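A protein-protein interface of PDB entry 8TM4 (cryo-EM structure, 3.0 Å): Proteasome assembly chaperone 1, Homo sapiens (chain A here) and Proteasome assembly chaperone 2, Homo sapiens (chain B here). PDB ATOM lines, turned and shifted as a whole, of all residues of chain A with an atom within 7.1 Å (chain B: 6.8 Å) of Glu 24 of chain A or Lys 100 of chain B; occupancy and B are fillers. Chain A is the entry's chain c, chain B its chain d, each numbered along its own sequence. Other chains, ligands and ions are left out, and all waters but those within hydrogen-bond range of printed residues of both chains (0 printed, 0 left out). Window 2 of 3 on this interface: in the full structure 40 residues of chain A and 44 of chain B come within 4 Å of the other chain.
The side-chain amino group of Lys 100 of chain B lies within hydrogen-bond range of the backbone carbonyl oxygen of Glu 24 of chain A.
OH of Tyr 97 of chain B sits close to NZ of Lys 96 of chain B (3.5 Å). O of Ser 99 of chain B is in hydrogen-bond range of SG of Cys 103 of chain B.
Glu 24 of chain A touches just these residues of chain B: Tyr 97 and Lys 100. Of the printed residues of chain B, Glu 21 of chain A touches Ser 99 (3.9 Å). Of the printed residues of chain B, Glu 25 of chain A touches Lys 100. Of the printed residues of chain A, Ser 99 of chain B touches Glu 21 (3.9 Å). Ile 186 of chain B touches none of the printed residues of chain A. Glu 23 of chain A touches none of the printed residues of chain B. The nearest residue of chain B that does not touch Glu 24 of chain A is Lys 96 of chain B (4.6 Å). The nearest printed residue of chain A that does not touch Ser 99 of chain B is Glu 24 of chain A (4.9 Å).
Among the printed residues, pairs that only touch across the chains: Arg 38 of chain A with Tyr 97 of chain B, Glu 24 of chain A with Tyr 97 of chain B, Glu 25 of chain A with Lys 100 of chain B and Glu 21 of chain A with Ser 99 of chain B.
Hydrophobic or aromatic side chains of chain B that line the printed part of chain A: Tyr 97. Of the 12 printed residues of chain A, 4 touch a printed residue of chain B. Among the printed residues, 5 pairs touch across the chains. Among the printed residues, no Asp or Glu carboxylate lies within 4 Å of a Lys or Arg side-chain nitrogen of the other chain.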
ATOM      1  N   THR A  18      -0.157  13.348   0.466  1.00  0.00           N
ATOM      2  CA  THR A  18       0.724  13.006   1.617  1.00  0.00           C
ATOM      3  C   THR A  18       0.268  13.767   2.867  1.00  0.00           C
ATOM      4  O   THR A  18       0.383  13.203   3.970  1.00  0.00           O
ATOM      5  CB  THR A  18       2.190  13.312   1.289  1.00  0.00           C
ATOM      6  OG1 THR A  18       2.259  14.655   0.805  1.00  0.00           O
ATOM      7  CG2 THR A  18       2.768  12.356   0.271  1.00  0.00           C
ATOM      8  N   GLU A  19      -0.223  14.996   2.689  1.00  0.00           N
ATOM      9  CA  GLU A  19      -0.921  15.793   3.736  1.00  0.00           C
ATOM     10  C   GLU A  19      -2.182  15.042   4.187  1.00  0.00           C
ATOM     11  O   GLU A  19      -2.527  15.143   5.380  1.00  0.00           O
ATOM     12  CB  GLU A  19      -1.230  17.216   3.246  1.00  0.00           C
ATOM     13  CG  GLU A  19      -2.390  17.349   2.260  1.00  0.00           C
ATOM     14  CD  GLU A  19      -2.206  16.737   0.881  1.00  0.00           C
ATOM     15  OE1 GLU A  19      -1.054  16.664   0.408  1.00  0.00           O
ATOM     16  OE2 GLU A  19      -3.221  16.333   0.280  1.00  0.00           O
ATOM     17  N   ASP A  20      -2.823  14.309   3.271  1.00  0.00           N
ATOM     18  CA  ASP A  20      -4.044  13.501   3.530  1.00  0.00           C
ATOM     19  C   ASP A  20      -3.652  12.240   4.308  1.00  0.00           C
ATOM     20  O   ASP A  20      -4.456  11.790   5.146  1.00  0.00           O
ATOM     21  CB  ASP A  20      -4.765  13.159   2.224  1.00  0.00           C
ATOM     22  N   GLU A  21      -2.454  11.709   4.040  1.00  0.00           N
ATOM     23  CA  GLU A  21      -1.838  10.568   4.768  1.00  0.00           C
ATOM     24  C   GLU A  21      -1.474  11.007   6.191  1.00  0.00           C
ATOM     25  O   GLU A  21      -1.540  10.160   7.104  1.00  0.00           O
ATOM     26  CB  GLU A  21      -0.602  10.069   4.016  1.00  0.00           C
ATOM     27  N   GLU A  22      -1.106  12.279   6.363  1.00  0.00           N
ATOM     28  CA  GLU A  22      -0.771  12.896   7.675  1.00  0.00           C
ATOM     29  C   GLU A  22      -2.062  13.123   8.468  1.00  0.00           C
ATOM     30  O   GLU A  22      -2.023  13.002   9.708  1.00  0.00           O
ATOM     31  CB  GLU A  22      -0.004  14.203   7.464  1.00  0.00           C
ATOM     32  N   GLU A  23      -3.161  13.432   7.771  1.00  0.00           N
ATOM     33  CA  GLU A  23      -4.523  13.550   8.355  1.00  0.00           C
ATOM     34  C   GLU A  23      -4.973  12.166   8.835  1.00  0.00           C
ATOM     35  O   GLU A  23      -5.578  12.085   9.921  1.00  0.00           O
ATOM     36  CB  GLU A  23      -5.496  14.135   7.330  1.00  0.00           C
ATOM     37  N   GLU A  24      -4.672  11.124   8.052  1.00  0.00           N
ATOM     38  CA  GLU A  24      -4.828   9.702   8.453  1.00  0.00           C
ATOM     39  C   GLU A  24      -4.147   9.510   9.810  1.00  0.00           C
ATOM     40  O   GLU A  24      -4.842   9.113  10.763  1.00  0.00           O
ATOM     41  CB  GLU A  24      -4.226   8.772   7.400  1.00  0.00           C
ATOM     42  N   GLU A  25      -2.843   9.802   9.882  1.00  0.00           N
ATOM     43  CA  GLU A  25      -2.021   9.722  11.119  1.00  0.00           C
ATOM     44  C   GLU A  25      -2.826  10.285  12.293  1.00  0.00           C
ATOM     45  O   GLU A  25      -3.020   9.548  13.281  1.00  0.00           O
ATOM     46  CB  GLU A  25      -0.702  10.476  10.939  1.00  0.00           C
ATOM     47  N   GLU A  26      -3.280  11.538  12.176  1.00  0.00           N
ATOM     48  CA  GLU A  26      -4.051  12.256  13.223  1.00  0.00           C
ATOM     49  C   GLU A  26      -5.237  11.392  13.666  1.00  0.00           C
ATOM     50  O   GLU A  26      -5.281  11.020  14.854  1.00  0.00           O
ATOM     51  CB  GLU A  26      -4.529  13.611  12.697  1.00  0.00           C
ATOM     52  N   GLY A  27      -6.152  11.084  12.740  1.00  0.00           N
ATOM     53  CA  GLY A  27      -7.508  10.584  13.034  1.00  0.00           C
ATOM     54  C   GLY A  27      -8.307  11.612  13.815  1.00  0.00           C
ATOM     55  O   GLY A  27      -9.095  11.208  14.693  1.00  0.00           O
ATOM     56  N   ARG A  28      -8.099  12.898  13.504  1.00  0.00           N
ATOM     57  CA  ARG A  28      -8.553  14.062  14.312  1.00  0.00           C
ATOM     58  C   ARG A  28      -8.054  13.892  15.751  1.00  0.00           C
ATOM     59  O   ARG A  28      -8.893  13.887  16.674  1.00  0.00           O
ATOM     60  CB  ARG A  28     -10.077  14.201  14.252  1.00  0.00           C
ATOM     61  N   ARG A  38     -16.226   8.931  11.727  1.00  0.00           N
ATOM     62  CA  ARG A  38     -15.566   8.404  10.499  1.00  0.00           C
ATOM     63  C   ARG A  38     -15.791   6.890  10.406  1.00  0.00           C
ATOM     64  O   ARG A  38     -15.607   6.347   9.304  1.00  0.00           O
ATOM     65  CB  ARG A  38     -14.077   8.768  10.438  1.00  0.00           C
ATOM     66  CG  ARG A  38     -13.207   8.115  11.500  1.00  0.00           C
ATOM     67  CD  ARG A  38     -11.728   8.226  11.190  1.00  0.00           C
ATOM     68  NE  ARG A  38     -10.893   7.998  12.364  1.00  0.00           N
ATOM     69  CZ  ARG A  38     -10.603   6.813  12.911  1.00  0.00           C
ATOM     70  NH1 ARG A  38     -11.082   5.680  12.415  1.00  0.00           N
ATOM     71  NH2 ARG A  38      -9.822   6.769  13.979  1.00  0.00           N
ATOM     72  N   CYS B  51      -4.182  -1.034   0.519  1.00  0.00           N
ATOM     73  CA  CYS B  51      -3.714   0.234   1.142  1.00  0.00           C
ATOM     74  C   CYS B  51      -3.381   1.287   0.078  1.00  0.00           C
ATOM     75  O   CYS B  51      -3.679   2.468   0.324  1.00  0.00           O
ATOM     76  CB  CYS B  51      -2.509  -0.017   2.040  1.00  0.00           C
ATOM     77  SG  CYS B  51      -2.867  -1.164   3.397  1.00  0.00           S
ATOM     78  N   PHE B  94      -2.396   6.723  -1.923  1.00  0.00           N
ATOM     79  CA  PHE B  94      -2.726   5.934  -0.710  1.00  0.00           C
ATOM     80  C   PHE B  94      -4.188   6.179  -0.328  1.00  0.00           C
ATOM     81  O   PHE B  94      -4.764   7.201  -0.751  1.00  0.00           O
ATOM     82  CB  PHE B  94      -1.763   6.261   0.434  1.00  0.00           C
ATOM     83  CG  PHE B  94      -0.660   5.248   0.593  1.00  0.00           C
ATOM     84  CD1 PHE B  94      -0.865   4.101   1.341  1.00  0.00           C
ATOM     85  CD2 PHE B  94       0.566   5.421  -0.028  1.00  0.00           C
ATOM     86  CE1 PHE B  94       0.139   3.160   1.480  1.00  0.00           C
ATOM     87  CE2 PHE B  94       1.568   4.475   0.111  1.00  0.00           C
ATOM     88  CZ  PHE B  94       1.354   3.348   0.865  1.00  0.00           C
ATOM     89  N   ILE B  95      -4.750   5.249   0.446  1.00  0.00           N
ATOM     90  CA  ILE B  95      -6.156   5.266   0.947  1.00  0.00           C
ATOM     91  C   ILE B  95      -6.094   5.718   2.410  1.00  0.00           C
ATOM     92  O   ILE B  95      -5.099   5.382   3.082  1.00  0.00           O
ATOM     93  CB  ILE B  95      -6.818   3.882   0.755  1.00  0.00           C
ATOM     94  CG1 ILE B  95      -6.869   3.496  -0.729  1.00  0.00           C
ATOM     95  CG2 ILE B  95      -8.197   3.836   1.404  1.00  0.00           C
ATOM     96  CD1 ILE B  95      -7.143   2.036  -1.001  1.00  0.00           C
ATOM     97  N   LYS B  96      -7.086   6.489   2.865  1.00  0.00           N
ATOM     98  CA  LYS B  96      -7.052   7.190   4.177  1.00  0.00           C
ATOM     99  C   LYS B  96      -7.319   6.168   5.290  1.00  0.00           C
ATOM    100  O   LYS B  96      -8.249   5.353   5.136  1.00  0.00           O
ATOM    101  CB  LYS B  96      -8.019   8.381   4.185  1.00  0.00           C
ATOM    102  CG  LYS B  96      -9.509   8.055   4.237  1.00  0.00           C
ATOM    103  CD  LYS B  96     -10.415   9.142   3.675  1.00  0.00           C
ATOM    104  CE  LYS B  96     -10.178  10.538   4.221  1.00  0.00           C
ATOM    105  NZ  LYS B  96     -10.301  10.608   5.698  1.00  0.00           N
ATOM    106  N   TYR B  97      -6.493   6.206   6.343  1.00  0.00           N
ATOM    107  CA  TYR B  97      -6.434   5.243   7.477  1.00  0.00           C
ATOM    108  C   TYR B  97      -6.003   3.857   6.978  1.00  0.00           C
ATOM    109  O   TYR B  97      -6.360   2.857   7.632  1.00  0.00           O
ATOM    110  CB  TYR B  97      -7.772   5.209   8.221  1.00  0.00           C
ATOM    111  CG  TYR B  97      -8.370   6.572   8.462  1.00  0.00           C
ATOM    112  CD1 TYR B  97      -7.743   7.485   9.291  1.00  0.00           C
ATOM    113  CD2 TYR B  97      -9.552   6.960   7.854  1.00  0.00           C
ATOM    114  CE1 TYR B  97      -8.275   8.743   9.516  1.00  0.00           C
ATOM    115  CE2 TYR B  97     -10.097   8.214   8.065  1.00  0.00           C
ATOM    116  CZ  TYR B  97      -9.453   9.114   8.896  1.00  0.00           C
ATOM    117  OH  TYR B  97      -9.967  10.358   9.126  1.00  0.00           O
ATOM    118  N   LYS B  98      -5.267   3.816   5.858  1.00  0.00           N
ATOM    119  CA  LYS B  98      -4.669   2.587   5.269  1.00  0.00           C
ATOM    120  C   LYS B  98      -3.142   2.728   5.139  1.00  0.00           C
ATOM    121  O   LYS B  98      -2.516   1.726   4.775  1.00  0.00           O
ATOM    122  CB  LYS B  98      -5.315   2.312   3.907  1.00  0.00           C
ATOM    123  CG  LYS B  98      -6.250   1.112   3.848  1.00  0.00           C
ATOM    124  CD  LYS B  98      -7.567   1.349   4.559  1.00  0.00           C
ATOM    125  CE  LYS B  98      -8.478   0.140   4.572  1.00  0.00           C
ATOM    126  NZ  LYS B  98      -8.033  -0.888   5.544  1.00  0.00           N
ATOM    127  N   SER B  99      -2.558   3.901   5.424  1.00  0.00           N
ATOM    128  CA  SER B  99      -1.122   4.215   5.206  1.00  0.00           C
ATOM    129  C   SER B  99      -0.275   3.581   6.315  1.00  0.00           C
ATOM    130  O   SER B  99       0.814   3.070   6.006  1.00  0.00           O
ATOM    131  CB  SER B  99      -0.899   5.700   5.125  1.00  0.00           C
ATOM    132  OG  SER B  99      -1.639   6.261   4.052  1.00  0.00           O
ATOM    133  N   LYS B 100      -0.768   3.618   7.555  1.00  0.00           N
ATOM    134  CA  LYS B 100      -0.095   3.020   8.740  1.00  0.00           C
ATOM    135  C   LYS B 100      -0.246   1.493   8.712  1.00  0.00           C
ATOM    136  O   LYS B 100       0.762   0.821   8.997  1.00  0.00           O
ATOM    137  CB  LYS B 100      -0.629   3.617  10.046  1.00  0.00           C
ATOM    138  CG  LYS B 100      -0.381   5.106  10.233  1.00  0.00           C
ATOM    139  CD  LYS B 100      -1.531   5.810  10.911  1.00  0.00           C
ATOM    140  CE  LYS B 100      -2.680   6.123   9.972  1.00  0.00           C
ATOM    141  NZ  LYS B 100      -3.954   6.305  10.705  1.00  0.00           N
ATOM    142  N   PRO B 101      -1.422   0.892   8.401  1.00  0.00           N
ATOM    143  CA  PRO B 101      -1.470  -0.521   8.022  1.00  0.00           C
ATOM    144  C   PRO B 101      -0.330  -0.903   7.067  1.00  0.00           C
ATOM    145  O   PRO B 101       0.383  -1.816   7.396  1.00  0.00           O
ATOM    146  CB  PRO B 101      -2.861  -0.666   7.394  1.00  0.00           C
ATOM    147  CG  PRO B 101      -3.697   0.265   8.233  1.00  0.00           C
ATOM    148  CD  PRO B 101      -2.784   1.442   8.518  1.00  0.00           C
ATOM    149  N   PHE B 102      -0.163  -0.192   5.946  1.00  0.00           N
ATOM    150  CA  PHE B 102       0.869  -0.501   4.920  1.00  0.00           C
ATOM    151  C   PHE B 102       2.253  -0.521   5.573  1.00  0.00           C
ATOM    152  O   PHE B 102       2.999  -1.490   5.354  1.00  0.00           O
ATOM    153  CB  PHE B 102       0.852   0.505   3.767  1.00  0.00           C
ATOM    154  CG  PHE B 102       1.968   0.316   2.770  1.00  0.00           C
ATOM    155  CD1 PHE B 102       3.206   0.912   2.962  1.00  0.00           C
ATOM    156  CD2 PHE B 102       1.782  -0.469   1.644  1.00  0.00           C
ATOM    157  CE1 PHE B 102       4.230   0.727   2.049  1.00  0.00           C
ATOM    158  CE2 PHE B 102       2.807  -0.649   0.730  1.00  0.00           C
ATOM    159  CZ  PHE B 102       4.028  -0.054   0.937  1.00  0.00           C
ATOM    160  N   CYS B 103       2.596   0.534   6.316  1.00  0.00           N
ATOM    161  CA  CYS B 103       3.909   0.679   6.996  1.00  0.00           C
ATOM    162  C   CYS B 103       4.158  -0.563   7.854  1.00  0.00           C
ATOM    163  O   CYS B 103       5.241  -1.161   7.731  1.00  0.00           O
ATOM    164  CB  CYS B 103       3.968   1.939   7.852  1.00  0.00           C
ATOM    165  SG  CYS B 103       3.880   3.465   6.881  1.00  0.00           S
ATOM    166  N   GLU B 104       3.166  -0.944   8.662  1.00  0.00           N
ATOM    167  CA  GLU B 104       3.215  -2.134   9.551  1.00  0.00           C
ATOM    168  C   GLU B 104       3.481  -3.374   8.692  1.00  0.00           C
ATOM    169  O   GLU B 104       4.440  -4.103   9.000  1.00  0.00           O
ATOM    170  CB  GLU B 104       1.915  -2.258  10.352  1.00  0.00           C
ATOM    171  CG  GLU B 104       1.905  -3.407  11.347  1.00  0.00           C
ATOM    172  CD  GLU B 104       2.894  -3.281  12.491  1.00  0.00           C
ATOM    173  OE1 GLU B 104       3.331  -4.330  13.007  1.00  0.00           O
ATOM    174  OE2 GLU B 104       3.215  -2.139  12.876  1.00  0.00           O
ATOM    175  N   LYS B 105       2.673  -3.582   7.647  1.00  0.00           N
ATOM    176  CA  LYS B 105       2.757  -4.764   6.745  1.00  0.00           C
ATOM    177  C   LYS B 105       4.199  -4.889   6.250  1.00  0.00           C
ATOM    178  O   LYS B 105       4.734  -6.004   6.296  1.00  0.00           O
ATOM    179  CB  LYS B 105       1.812  -4.651   5.542  1.00  0.00           C
ATOM    180  CG  LYS B 105       0.329  -4.507   5.866  1.00  0.00           C
ATOM    181  CD  LYS B 105      -0.579  -5.439   5.093  1.00  0.00           C
ATOM    182  CE  LYS B 105      -2.025  -5.381   5.543  1.00  0.00           C
ATOM    183  NZ  LYS B 105      -2.679  -4.089   5.216  1.00  0.00           N
ATOM    184  N   ILE B 186       3.800   8.493   4.040  1.00  0.00           N
ATOM    185  CA  ILE B 186       3.976   7.183   4.733  1.00  0.00           C
ATOM    186  C   ILE B 186       5.403   7.085   5.289  1.00  0.00           C
ATOM    187  O   ILE B 186       5.625   6.167   6.061  1.00  0.00           O
ATOM    188  CB  ILE B 186       3.647   6.005   3.791  1.00  0.00           C
ATOM    189  CG1 ILE B 186       4.826   5.649   2.874  1.00  0.00           C
ATOM    190  CG2 ILE B 186       2.364   6.287   3.016  1.00  0.00           C
ATOM    191  CD1 ILE B 186       4.501   4.656   1.789  1.00  0.00           C
ATOM    192  N   THR B 189       5.781   7.873   9.350  1.00  0.00           N
ATOM    193  CA  THR B 189       5.186   6.783  10.171  1.00  0.00           C
ATOM    194  C   THR B 189       6.027   5.511  10.028  1.00  0.00           C
ATOM    195  O   THR B 189       6.154   4.782  11.025  1.00  0.00           O
ATOM    196  CB  THR B 189       3.721   6.531   9.789  1.00  0.00           C
ATOM    197  OG1 THR B 189       3.618   6.544   8.365  1.00  0.00           O
ATOM    198  CG2 THR B 189       2.773   7.555  10.372  1.00  0.00           C
ATOM    199  N   GLU B 193       7.845   3.582  13.097  1.00  0.00           N
ATOM    200  CA  GLU B 193       7.498   2.153  13.312  1.00  0.00           C
ATOM    201  C   GLU B 193       8.767   1.307  13.180  1.00  0.00           C
ATOM    202  O   GLU B 193       8.888   0.330  13.921  1.00  0.00           O
ATOM    203  CB  GLU B 193       6.420   1.691  12.331  1.00  0.00           C
ATOM    204  CG  GLU B 193       5.019   2.159  12.681  1.00  0.00           C
ATOM    205  CD  GLU B 193       4.262   1.264  13.649  1.00  0.00           C
ATOM    206  OE1 GLU B 193       3.016   1.292  13.617  1.00  0.00           O
ATOM    207  OE2 GLU B 193       4.913   0.548  14.437  1.00  0.00           O
